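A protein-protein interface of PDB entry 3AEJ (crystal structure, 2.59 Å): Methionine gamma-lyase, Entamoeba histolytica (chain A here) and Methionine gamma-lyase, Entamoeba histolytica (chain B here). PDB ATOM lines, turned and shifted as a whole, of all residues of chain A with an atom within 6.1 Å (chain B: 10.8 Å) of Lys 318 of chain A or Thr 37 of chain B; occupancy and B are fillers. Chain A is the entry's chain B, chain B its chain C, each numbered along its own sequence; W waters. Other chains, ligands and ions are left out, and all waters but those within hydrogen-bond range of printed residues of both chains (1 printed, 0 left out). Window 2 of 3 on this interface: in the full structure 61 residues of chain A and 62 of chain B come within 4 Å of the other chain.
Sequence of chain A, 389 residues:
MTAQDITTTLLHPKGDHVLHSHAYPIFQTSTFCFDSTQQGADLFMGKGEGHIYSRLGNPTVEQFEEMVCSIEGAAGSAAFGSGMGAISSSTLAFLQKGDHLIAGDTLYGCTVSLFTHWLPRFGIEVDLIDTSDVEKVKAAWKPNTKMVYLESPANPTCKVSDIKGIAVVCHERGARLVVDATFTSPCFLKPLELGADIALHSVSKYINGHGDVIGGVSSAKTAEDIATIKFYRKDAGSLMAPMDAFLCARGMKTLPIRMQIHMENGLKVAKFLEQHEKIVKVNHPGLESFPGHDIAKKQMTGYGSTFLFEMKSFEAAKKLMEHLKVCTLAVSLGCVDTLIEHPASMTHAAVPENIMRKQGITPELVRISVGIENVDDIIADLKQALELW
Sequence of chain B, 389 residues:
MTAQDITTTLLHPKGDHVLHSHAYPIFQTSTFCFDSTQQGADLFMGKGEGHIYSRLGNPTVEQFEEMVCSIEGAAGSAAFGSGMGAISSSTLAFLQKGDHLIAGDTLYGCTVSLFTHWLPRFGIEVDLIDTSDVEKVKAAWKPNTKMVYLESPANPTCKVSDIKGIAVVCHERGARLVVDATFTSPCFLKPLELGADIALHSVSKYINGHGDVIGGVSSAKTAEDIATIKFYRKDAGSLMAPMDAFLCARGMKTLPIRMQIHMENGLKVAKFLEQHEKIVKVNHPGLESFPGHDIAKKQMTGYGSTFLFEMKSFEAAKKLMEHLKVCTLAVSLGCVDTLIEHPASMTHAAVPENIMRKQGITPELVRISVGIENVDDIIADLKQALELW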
ATOM      1  N   SER A 313      13.279  17.774 -12.945  1.00  0.00           N
ATOM      2  CA  SER A 313      12.305  16.719 -12.652  1.00  0.00           C
ATOM      3  C   SER A 313      11.451  17.065 -11.431  1.00  0.00           C
ATOM      4  O   SER A 313      11.631  18.120 -10.818  1.00  0.00           O
ATOM      5  CB  SER A 313      13.010  15.374 -12.444  1.00  0.00           C
ATOM      6  OG  SER A 313      13.843  15.402 -11.299  1.00  0.00           O
ATOM      7  N   PHE A 314      10.521  16.173 -11.091  1.00  0.00           N
ATOM      8  CA  PHE A 314       9.690  16.332  -9.898  1.00  0.00           C
ATOM      9  C   PHE A 314      10.497  16.126  -8.616  1.00  0.00           C
ATOM     10  O   PHE A 314      10.311  16.858  -7.641  1.00  0.00           O
ATOM     11  CB  PHE A 314       8.480  15.390  -9.938  1.00  0.00           C
ATOM     12  CG  PHE A 314       7.711  15.325  -8.644  1.00  0.00           C
ATOM     13  CD1 PHE A 314       7.678  14.149  -7.899  1.00  0.00           C
ATOM     14  CD2 PHE A 314       7.028  16.440  -8.163  1.00  0.00           C
ATOM     15  CE1 PHE A 314       6.973  14.081  -6.699  1.00  0.00           C
ATOM     16  CE2 PHE A 314       6.321  16.383  -6.962  1.00  0.00           C
ATOM     17  CZ  PHE A 314       6.294  15.201  -6.230  1.00  0.00           C
ATOM     18  N   GLU A 315      11.386  15.132  -8.627  1.00  0.00           N
ATOM     19  CA  GLU A 315      12.279  14.855  -7.498  1.00  0.00           C
ATOM     20  C   GLU A 315      13.221  16.021  -7.201  1.00  0.00           C
ATOM     21  O   GLU A 315      13.495  16.319  -6.037  1.00  0.00           O
ATOM     22  CB  GLU A 315      13.081  13.569  -7.732  1.00  0.00           C
ATOM     23  CG  GLU A 315      12.618  12.370  -6.902  1.00  0.00           C
ATOM     24  CD  GLU A 315      11.244  11.851  -7.299  1.00  0.00           C
ATOM     25  OE1 GLU A 315      10.311  11.949  -6.471  1.00  0.00           O
ATOM     26  OE2 GLU A 315      11.095  11.346  -8.433  1.00  0.00           O
ATOM     27  N   ALA A 316      13.705  16.670  -8.259  1.00  0.00           N
ATOM     28  CA  ALA A 316      14.544  17.864  -8.137  1.00  0.00           C
ATOM     29  C   ALA A 316      13.766  19.018  -7.507  1.00  0.00           C
ATOM     30  O   ALA A 316      14.281  19.720  -6.635  1.00  0.00           O
ATOM     31  CB  ALA A 316      15.097  18.268  -9.497  1.00  0.00           C
ATOM     32  N   ALA A 317      12.524  19.200  -7.955  1.00  0.00           N
ATOM     33  CA  ALA A 317      11.620  20.200  -7.391  1.00  0.00           C
ATOM     34  C   ALA A 317      11.309  19.893  -5.927  1.00  0.00           C
ATOM     35  O   ALA A 317      11.300  20.794  -5.085  1.00  0.00           O
ATOM     36  CB  ALA A 317      10.339  20.270  -8.207  1.00  0.00           C
ATOM     37  N   LYS A 318      11.066  18.614  -5.643  1.00  0.00           N
ATOM     38  CA  LYS A 318      10.811  18.117  -4.289  1.00  0.00           C
ATOM     39  C   LYS A 318      11.972  18.433  -3.343  1.00  0.00           C
ATOM     40  O   LYS A 318      11.753  18.921  -2.233  1.00  0.00           O
ATOM     41  CB  LYS A 318      10.549  16.605  -4.334  1.00  0.00           C
ATOM     42  CG  LYS A 318      10.278  15.939  -2.992  1.00  0.00           C
ATOM     43  CD  LYS A 318      10.494  14.432  -3.092  1.00  0.00           C
ATOM     44  CE  LYS A 318      10.210  13.724  -1.775  1.00  0.00           C
ATOM     45  NZ  LYS A 318       8.751  13.563  -1.527  1.00  0.00           N
ATOM     46  N   LYS A 319      13.197  18.160  -3.792  1.00  0.00           N
ATOM     47  CA  LYS A 319      14.404  18.398  -2.993  1.00  0.00           C
ATOM     48  C   LYS A 319      14.624  19.878  -2.678  1.00  0.00           C
ATOM     49  O   LYS A 319      15.062  20.222  -1.578  1.00  0.00           O
ATOM     50  CB  LYS A 319      15.640  17.823  -3.689  1.00  0.00           C
ATOM     51  CG  LYS A 319      15.811  16.322  -3.530  1.00  0.00           C
ATOM     52  CD  LYS A 319      17.091  15.846  -4.201  1.00  0.00           C
ATOM     53  CE  LYS A 319      17.277  14.345  -4.044  1.00  0.00           C
ATOM     54  NZ  LYS A 319      18.500  13.861  -4.743  1.00  0.00           N
ATOM     55  N   LEU A 320      14.322  20.742  -3.646  1.00  0.00           N
ATOM     56  CA  LEU A 320      14.473  22.185  -3.473  1.00  0.00           C
ATOM     57  C   LEU A 320      13.506  22.735  -2.426  1.00  0.00           C
ATOM     58  O   LEU A 320      13.918  23.447  -1.513  1.00  0.00           O
ATOM     59  CB  LEU A 320      14.296  22.917  -4.812  1.00  0.00           C
ATOM     60  CG  LEU A 320      14.246  24.453  -4.816  1.00  0.00           C
ATOM     61  CD1 LEU A 320      15.564  25.076  -4.361  1.00  0.00           C
ATOM     62  CD2 LEU A 320      13.859  24.970  -6.192  1.00  0.00           C
ATOM     63  N   MET A 321      12.229  22.384  -2.561  1.00  0.00           N
ATOM     64  CA  MET A 321      11.171  22.900  -1.689  1.00  0.00           C
ATOM     65  C   MET A 321      11.258  22.412  -0.244  1.00  0.00           C
ATOM     66  O   MET A 321      10.775  23.084   0.671  1.00  0.00           O
ATOM     67  CB  MET A 321       9.794  22.554  -2.261  1.00  0.00           C
ATOM     68  CG  MET A 321       9.420  23.321  -3.520  1.00  0.00           C
ATOM     69  SD  MET A 321       7.756  22.931  -4.095  1.00  0.00           S
ATOM     70  CE  MET A 321       7.988  21.283  -4.759  1.00  0.00           C
ATOM     71  N   GLU A 322      11.872  21.249  -0.046  1.00  0.00           N
ATOM     72  CA  GLU A 322      11.919  20.610   1.270  1.00  0.00           C
ATOM     73  C   GLU A 322      13.216  20.853   2.047  1.00  0.00           C
ATOM     74  O   GLU A 322      13.338  20.428   3.199  1.00  0.00           O
ATOM     75  CB  GLU A 322      11.662  19.106   1.138  1.00  0.00           C
ATOM     76  CG  GLU A 322      10.237  18.749   0.738  1.00  0.00           C
ATOM     77  CD  GLU A 322      10.017  17.255   0.620  1.00  0.00           C
ATOM     78  OE1 GLU A 322      10.983  16.518   0.323  1.00  0.00           O
ATOM     79  OE2 GLU A 322       8.870  16.812   0.823  1.00  0.00           O
ATOM     80  N   HIS A 323      14.176  21.535   1.423  1.00  0.00           N
ATOM     81  CA  HIS A 323      15.461  21.816   2.069  1.00  0.00           C
ATOM     82  C   HIS A 323      15.815  23.307   2.105  1.00  0.00           C
ATOM     83  O   HIS A 323      16.986  23.684   2.001  1.00  0.00           O
ATOM     84  CB  HIS A 323      16.579  20.994   1.423  1.00  0.00           C
ATOM     85  CG  HIS A 323      16.449  19.521   1.650  1.00  0.00           C
ATOM     86  ND1 HIS A 323      15.931  18.664   0.703  1.00  0.00           N
ATOM     87  CD2 HIS A 323      16.762  18.753   2.721  1.00  0.00           C
ATOM     88  CE1 HIS A 323      15.936  17.430   1.178  1.00  0.00           C
ATOM     89  NE2 HIS A 323      16.435  17.458   2.401  1.00  0.00           N
ATOM     90  N   LEU A 329       7.632  26.855   2.927  1.00  0.00           N
ATOM     91  CA  LEU A 329       6.745  26.095   2.052  1.00  0.00           C
ATOM     92  C   LEU A 329       5.292  26.293   2.478  1.00  0.00           C
ATOM     93  O   LEU A 329       4.840  25.732   3.483  1.00  0.00           O
ATOM     94  CB  LEU A 329       7.127  24.608   2.042  1.00  0.00           C
ATOM     95  CG  LEU A 329       6.369  23.658   1.104  1.00  0.00           C
ATOM     96  CD1 LEU A 329       6.623  23.984  -0.368  1.00  0.00           C
ATOM     97  CD2 LEU A 329       6.743  22.212   1.402  1.00  0.00           C
ATOM     98  N   HIS A 342       4.055  24.465  -4.711  1.00  0.00           N
ATOM     99  CA  HIS A 342       4.014  23.518  -5.827  1.00  0.00           C
ATOM    100  C   HIS A 342       2.630  23.513  -6.486  1.00  0.00           C
ATOM    101  O   HIS A 342       1.717  22.840  -6.003  1.00  0.00           O
ATOM    102  CB  HIS A 342       4.391  22.112  -5.349  1.00  0.00           C
ATOM    103  CG  HIS A 342       4.353  21.071  -6.426  1.00  0.00           C
ATOM    104  ND1 HIS A 342       5.406  20.850  -7.286  1.00  0.00           N
ATOM    105  CD2 HIS A 342       3.390  20.187  -6.774  1.00  0.00           C
ATOM    106  CE1 HIS A 342       5.091  19.875  -8.121  1.00  0.00           C
ATOM    107  NE2 HIS A 342       3.873  19.455  -7.831  1.00  0.00           N
ATOM    108  N   SER A 345       0.181  20.194  -7.420  1.00  0.00           N
ATOM    109  CA  SER A 345      -0.465  19.453  -6.339  1.00  0.00           C
ATOM    110  C   SER A 345      -0.984  20.337  -5.200  1.00  0.00           C
ATOM    111  O   SER A 345      -1.401  19.828  -4.155  1.00  0.00           O
ATOM    112  CB  SER A 345       0.475  18.367  -5.799  1.00  0.00           C
ATOM    113  OG  SER A 345       1.502  18.923  -4.996  1.00  0.00           O
ATOM    114  N   MET A 346      -0.973  21.654  -5.407  1.00  0.00           N
ATOM    115  CA  MET A 346      -1.461  22.595  -4.391  1.00  0.00           C
ATOM    116  C   MET A 346      -2.482  23.606  -4.934  1.00  0.00           C
ATOM    117  O   MET A 346      -3.672  23.293  -5.013  1.00  0.00           O
ATOM    118  CB  MET A 346      -0.296  23.292  -3.675  1.00  0.00           C
ATOM    119  CG  MET A 346       0.540  22.369  -2.798  1.00  0.00           C
ATOM    120  SD  MET A 346       2.150  23.052  -2.371  1.00  0.00           S
ATOM    121  CE  MET A 346       2.891  21.657  -1.524  1.00  0.00           C
ATOM    122  N   VAL A 366       7.770  25.172 -10.148  1.00  0.00           N
ATOM    123  CA  VAL A 366       7.770  25.673  -8.773  1.00  0.00           C
ATOM    124  C   VAL A 366       7.500  27.180  -8.755  1.00  0.00           C
ATOM    125  O   VAL A 366       8.103  27.935  -9.519  1.00  0.00           O
ATOM    126  CB  VAL A 366       9.109  25.360  -8.049  1.00  0.00           C
ATOM    127  CG1 VAL A 366       9.135  25.966  -6.650  1.00  0.00           C
ATOM    128  CG2 VAL A 366       9.341  23.860  -7.971  1.00  0.00           C
ATOM    129  N   PHE B  32      -1.003  28.795   5.961  1.00  0.00           N
ATOM    130  CA  PHE B  32      -0.396  27.865   6.906  1.00  0.00           C
ATOM    131  C   PHE B  32       0.821  27.176   6.289  1.00  0.00           C
ATOM    132  O   PHE B  32       0.905  27.029   5.072  1.00  0.00           O
ATOM    133  CB  PHE B  32      -1.428  26.835   7.368  1.00  0.00           C
ATOM    134  CG  PHE B  32      -2.470  27.395   8.297  1.00  0.00           C
ATOM    135  CD1 PHE B  32      -3.597  28.040   7.799  1.00  0.00           C
ATOM    136  CD2 PHE B  32      -2.324  27.272   9.675  1.00  0.00           C
ATOM    137  CE1 PHE B  32      -4.558  28.560   8.656  1.00  0.00           C
ATOM    138  CE2 PHE B  32      -3.278  27.789  10.543  1.00  0.00           C
ATOM    139  CZ  PHE B  32      -4.398  28.433  10.032  1.00  0.00           C
ATOM    140  N   CYS B  33       1.760  26.758   7.135  1.00  0.00           N
ATOM    141  CA  CYS B  33       3.012  26.146   6.682  1.00  0.00           C
ATOM    142  C   CYS B  33       2.883  24.633   6.513  1.00  0.00           C
ATOM    143  O   CYS B  33       2.206  23.970   7.299  1.00  0.00           O
ATOM    144  CB  CYS B  33       4.143  26.458   7.665  1.00  0.00           C
ATOM    145  SG  CYS B  33       4.270  28.198   8.153  1.00  0.00           S
ATOM    146  N   PHE B  34       3.539  24.093   5.490  1.00  0.00           N
ATOM    147  CA  PHE B  34       3.559  22.650   5.264  1.00  0.00           C
ATOM    148  C   PHE B  34       4.838  22.013   5.805  1.00  0.00           C
ATOM    149  O   PHE B  34       5.910  22.624   5.764  1.00  0.00           O
ATOM    150  CB  PHE B  34       3.407  22.318   3.773  1.00  0.00           C
ATOM    151  CG  PHE B  34       2.095  22.754   3.172  1.00  0.00           C
ATOM    152  CD1 PHE B  34       0.895  22.589   3.866  1.00  0.00           C
ATOM    153  CD2 PHE B  34       2.057  23.306   1.895  1.00  0.00           C
ATOM    154  CE1 PHE B  34      -0.320  22.988   3.303  1.00  0.00           C
ATOM    155  CE2 PHE B  34       0.850  23.705   1.321  1.00  0.00           C
ATOM    156  CZ  PHE B  34      -0.343  23.544   2.029  1.00  0.00           C
ATOM    157  N   ASP B  35       4.715  20.788   6.311  1.00  0.00           N
ATOM    158  CA  ASP B  35       5.871  20.014   6.763  1.00  0.00           C
ATOM    159  C   ASP B  35       6.685  19.516   5.571  1.00  0.00           C
ATOM    160  O   ASP B  35       7.917  19.500   5.608  1.00  0.00           O
ATOM    161  CB  ASP B  35       5.427  18.823   7.621  1.00  0.00           C
ATOM    162  CG  ASP B  35       4.782  19.246   8.931  1.00  0.00           C
ATOM    163  OD1 ASP B  35       5.249  20.225   9.554  1.00  0.00           O
ATOM    164  OD2 ASP B  35       3.807  18.586   9.347  1.00  0.00           O
ATOM    165  N   SER B  36       5.975  19.113   4.518  1.00  0.00           N
ATOM    166  CA  SER B  36       6.577  18.581   3.300  1.00  0.00           C
ATOM    167  C   SER B  36       5.637  18.797   2.119  1.00  0.00           C
ATOM    168  O   SER B  36       4.466  19.136   2.306  1.00  0.00           O
ATOM    169  CB  SER B  36       6.879  17.090   3.463  1.00  0.00           C
ATOM    170  OG  SER B  36       5.696  16.353   3.718  1.00  0.00           O
ATOM    171  N   THR B  37       6.151  18.599   0.906  1.00  0.00           N
ATOM    172  CA  THR B  37       5.345  18.738  -0.311  1.00  0.00           C
ATOM    173  C   THR B  37       4.194  17.725  -0.369  1.00  0.00           C
ATOM    174  O   THR B  37       3.117  18.040  -0.876  1.00  0.00           O
ATOM    175  CB  THR B  37       6.210  18.688  -1.608  1.00  0.00           C
ATOM    176  OG1 THR B  37       5.366  18.795  -2.761  1.00  0.00           O
ATOM    177  CG2 THR B  37       7.016  17.401  -1.699  1.00  0.00           C
ATOM    178  N   GLN B  38       4.428  16.526   0.165  1.00  0.00           N
ATOM    179  CA  GLN B  38       3.411  15.473   0.217  1.00  0.00           C
ATOM    180  C   GLN B  38       2.291  15.823   1.196  1.00  0.00           C
ATOM    181  O   GLN B  38       1.111  15.691   0.866  1.00  0.00           O
ATOM    182  CB  GLN B  38       4.044  14.126   0.589  1.00  0.00           C
ATOM    183  CG  GLN B  38       3.084  12.933   0.591  1.00  0.00           C
ATOM    184  CD  GLN B  38       2.736  12.439  -0.804  1.00  0.00           C
ATOM    185  OE1 GLN B  38       3.238  11.406  -1.250  1.00  0.00           O
ATOM    186  NE2 GLN B  38       1.874  13.175  -1.500  1.00  0.00           N
ATOM    187  N   GLN B  39       2.674  16.268   2.392  1.00  0.00           N
ATOM    188  CA  GLN B  39       1.727  16.672   3.431  1.00  0.00           C
ATOM    189  C   GLN B  39       0.836  17.826   2.957  1.00  0.00           C
ATOM    190  O   GLN B  39      -0.346  17.886   3.303  1.00  0.00           O
ATOM    191  CB  GLN B  39       2.482  17.037   4.717  1.00  0.00           C
ATOM    192  CG  GLN B  39       1.608  17.305   5.943  1.00  0.00           C
ATOM    193  CD  GLN B  39       1.442  18.789   6.256  1.00  0.00           C
ATOM    194  OE1 GLN B  39       0.947  19.153   7.324  1.00  0.00           O
ATOM    195  NE2 GLN B  39       1.862  19.649   5.333  1.00  0.00           N
ATOM    196  N   GLY B  40       1.411  18.726   2.160  1.00  0.00           N
ATOM    197  CA  GLY B  40       0.662  19.814   1.532  1.00  0.00           C
ATOM    198  C   GLY B  40      -0.250  19.322   0.421  1.00  0.00           C
ATOM    199  O   GLY B  40      -1.399  19.756   0.316  1.00  0.00           O
ATOM    200  N   ALA B  41       0.265  18.413  -0.404  1.00  0.00           N
ATOM    201  CA  ALA B  41      -0.517  17.799  -1.479  1.00  0.00           C
ATOM    202  C   ALA B  41      -1.697  17.001  -0.930  1.00  0.00           C
ATOM    203  O   ALA B  41      -2.790  17.032  -1.499  1.00  0.00           O
ATOM    204  CB  ALA B  41       0.369  16.909  -2.342  1.00  0.00           C
ATOM    205  N   ASP B  42      -1.462  16.299   0.179  1.00  0.00           N
ATOM    206  CA  ASP B  42      -2.483  15.474   0.821  1.00  0.00           C
ATOM    207  C   ASP B  42      -3.633  16.296   1.399  1.00  0.00           C
ATOM    208  O   ASP B  42      -4.795  15.904   1.282  1.00  0.00           O
ATOM    209  CB  ASP B  42      -1.860  14.591   1.911  1.00  0.00           C
ATOM    210  CG  ASP B  42      -1.091  13.402   1.346  1.00  0.00           C
ATOM    211  OD1 ASP B  42      -0.926  13.307   0.109  1.00  0.00           O
ATOM    212  OD2 ASP B  42      -0.647  12.555   2.148  1.00  0.00           O
ATOM    213  N   LEU B  43      -3.302  17.435   2.009  1.00  0.00           N
ATOM    214  CA  LEU B  43      -4.307  18.317   2.608  1.00  0.00           C
ATOM    215  C   LEU B  43      -5.275  18.901   1.579  1.00  0.00           C
ATOM    216  O   LEU B  43      -6.434  19.174   1.898  1.00  0.00           O
ATOM    217  CB  LEU B  43      -3.643  19.433   3.424  1.00  0.00           C
ATOM    218  CG  LEU B  43      -3.056  19.072   4.794  1.00  0.00           C
ATOM    219  CD1 LEU B  43      -2.267  20.241   5.369  1.00  0.00           C
ATOM    220  CD2 LEU B  43      -4.132  18.618   5.776  1.00  0.00           C
ATOM    221  N   PHE B  44      -4.793  19.090   0.352  1.00  0.00           N
ATOM    222  CA  PHE B  44      -5.640  19.514  -0.765  1.00  0.00           C
ATOM    223  C   PHE B  44      -6.534  18.377  -1.258  1.00  0.00           C
ATOM    224  O   PHE B  44      -7.650  18.617  -1.723  1.00  0.00           O
ATOM    225  CB  PHE B  44      -4.790  20.054  -1.919  1.00  0.00           C
ATOM    226  CG  PHE B  44      -4.432  21.510  -1.781  1.00  0.00           C
ATOM    227  CD1 PHE B  44      -3.219  21.893  -1.219  1.00  0.00           C
ATOM    228  CD2 PHE B  44      -5.308  22.500  -2.221  1.00  0.00           C
ATOM    229  CE1 PHE B  44      -2.884  23.237  -1.094  1.00  0.00           C
ATOM    230  CE2 PHE B  44      -4.983  23.847  -2.100  1.00  0.00           C
ATOM    231  CZ  PHE B  44      -3.768  24.216  -1.538  1.00  0.00           C
ATOM    232  N   MET B  45      -6.034  17.146  -1.150  1.00  0.00           N
ATOM    233  CA  MET B  45      -6.792  15.950  -1.526  1.00  0.00           C
ATOM    234  C   MET B  45      -7.873  15.598  -0.500  1.00  0.00           C
ATOM    235  O   MET B  45      -8.841  14.904  -0.824  1.00  0.00           O
ATOM    236  CB  MET B  45      -5.852  14.754  -1.715  1.00  0.00           C
ATOM    237  CG  MET B  45      -4.913  14.858  -2.911  1.00  0.00           C
ATOM    238  SD  MET B  45      -5.739  14.677  -4.503  1.00  0.00           S
ATOM    239  CE  MET B  45      -6.001  12.903  -4.572  1.00  0.00           C
ATOM    240  N   LYS B  47      -6.930  14.226   2.572  1.00  0.00           N
ATOM    241  CA  LYS B  47      -6.278  13.284   3.484  1.00  0.00           C
ATOM    242  C   LYS B  47      -5.352  13.986   4.473  1.00  0.00           C
ATOM    243  O   LYS B  47      -4.647  14.934   4.116  1.00  0.00           O
ATOM    244  CB  LYS B  47      -5.507  12.213   2.704  1.00  0.00           C
ATOM    245  CG  LYS B  47      -6.320  10.958   2.383  1.00  0.00           C
ATOM    246  CD  LYS B  47      -7.100  11.068   1.072  1.00  0.00           C
ATOM    247  CE  LYS B  47      -6.264  10.618  -0.121  1.00  0.00           C
ATOM    248  NZ  LYS B  47      -7.084  10.502  -1.358  1.00  0.00           N
ATOM    249  N   ILE B  52      -4.578  24.663   5.583  1.00  0.00           N
ATOM    250  CA  ILE B  52      -3.918  25.138   4.370  1.00  0.00           C
ATOM    251  C   ILE B  52      -3.961  26.664   4.299  1.00  0.00           C
ATOM    252  O   ILE B  52      -2.924  27.327   4.247  1.00  0.00           O
ATOM    253  CB  ILE B  52      -4.597  24.580   3.087  1.00  0.00           C
ATOM    254  CG1 ILE B  52      -4.582  23.049   3.071  1.00  0.00           C
ATOM    255  CG2 ILE B  52      -3.925  25.142   1.835  1.00  0.00           C
ATOM    256  CD1 ILE B  52      -5.528  22.434   2.052  1.00  0.00           C
HETATM  257  O   HOH W   1       7.272  14.792   0.435  1.00  0.00           O
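The backbone carbonyl oxygen (O) of Leu 329 of chain A is in hydrogen-bond range of the backbone NH (N) of Phe 34 of chain B, at 2.9 Å. The backbone NH of Thr 37 of chain B sits close to the side-chain carboxylate of Glu 322 of chain A (3.3 Å).
N of His 342 of chain A is in hydrogen-bond range of SD of Met 346 of chain A (3.3 Å). The side-chain hydroxyl (OG) of Ser 36 of chain B lies within hydrogen-bond range of the backbone NH (N) of Gln 39 of chain B, 3.3 Å away.
CG2 of Thr 37 of chain B touches CG of Lys 318 of chain A (3.8 Å). OE2 of Glu 322 of chain A touches CB of Ser 36 of chain B, 3.3 Å away. Cys 33 of chain B touches Leu 329 of chain A. Leu 329 of chain A touches Ser 36 of chain B. Thr 37 of chain B touches Leu 329 of chain A. Ala 41 of chain B touches Ser 345 of chain A. Met 346 of chain A touches Phe 34 of chain B (CE to CD2, 3.9 Å). Thr 37 of chain B touches Met 346 of chain A. Phe 44 of chain B touches Met 346 of chain A (CE2 to O, 3.2 Å).
Of the printed residues of chain B, Lys 318 of chain A touches Thr 37 (3.8 Å). Thr 37 of chain B touches four residues of chain A. No residue of chain B comes within 4 Å of Phe 314 of chain A. No residue of chain B comes within 4 Å of Ala 316 of chain A. No residue of chain B comes within 4 Å of Ala 317 of chain A. Of the printed residues of chain B, Glu 322 of chain A touches Ser 36 (3.3 Å) and Thr 37 (3.2 Å). Of the printed residues of chain A, Cys 33 of chain B touches Leu 329 (3.7 Å). Of the printed residues of chain B, Ser 345 of chain A touches Ala 41 (3.5 Å). Of the printed residues of chain A, Phe 44 of chain B touches Met 346. Of the printed residues of chain B, Met 346 of chain A touches Phe 34, Thr 37 and Phe 44. Val 366 of chain A touches none of the printed residues of chain B. The nearest residue of chain A that does not touch Thr 37 of chain B is Met 321 of chain A (4.1 Å). The nearest printed residue of chain A that does not touch Ser 36 of chain B is Met 346 of chain A (4.8 Å).
Printed residues of chain A that touch a printed residue of chain B: Lys 318, Glu 322, Leu 329, Ser 345 and Met 346. Hydrophobic or aromatic side chains of chain A within 4 Å of the printed part of chain B: Leu 329 and Met 346. Of the 16 printed residues of chain B, 6 touch a printed residue of chain A. Printed residues of chain B that touch a printed residue of chain A: Cys 33, Phe 34, Ser 36, Thr 37, Ala 41 and Phe 44. Hydrophobic or aromatic side chains of chain B that line the printed part of chain A: Phe 34, Ala 41 and Phe 44. Among the printed residues, 11 pairs touch across the chains. Among the printed residues, no Asp or Glu carboxylate lies within 4 Å of a Lys or Arg side-chain nitrogen of the other chain.
Water W1 lies within hydrogen-bond range of the side-chain carboxylate of Glu 322 of chain A, the side-chain amino group of Lys 318 of chain A and the backbone NH of Gln 38 of chain B.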
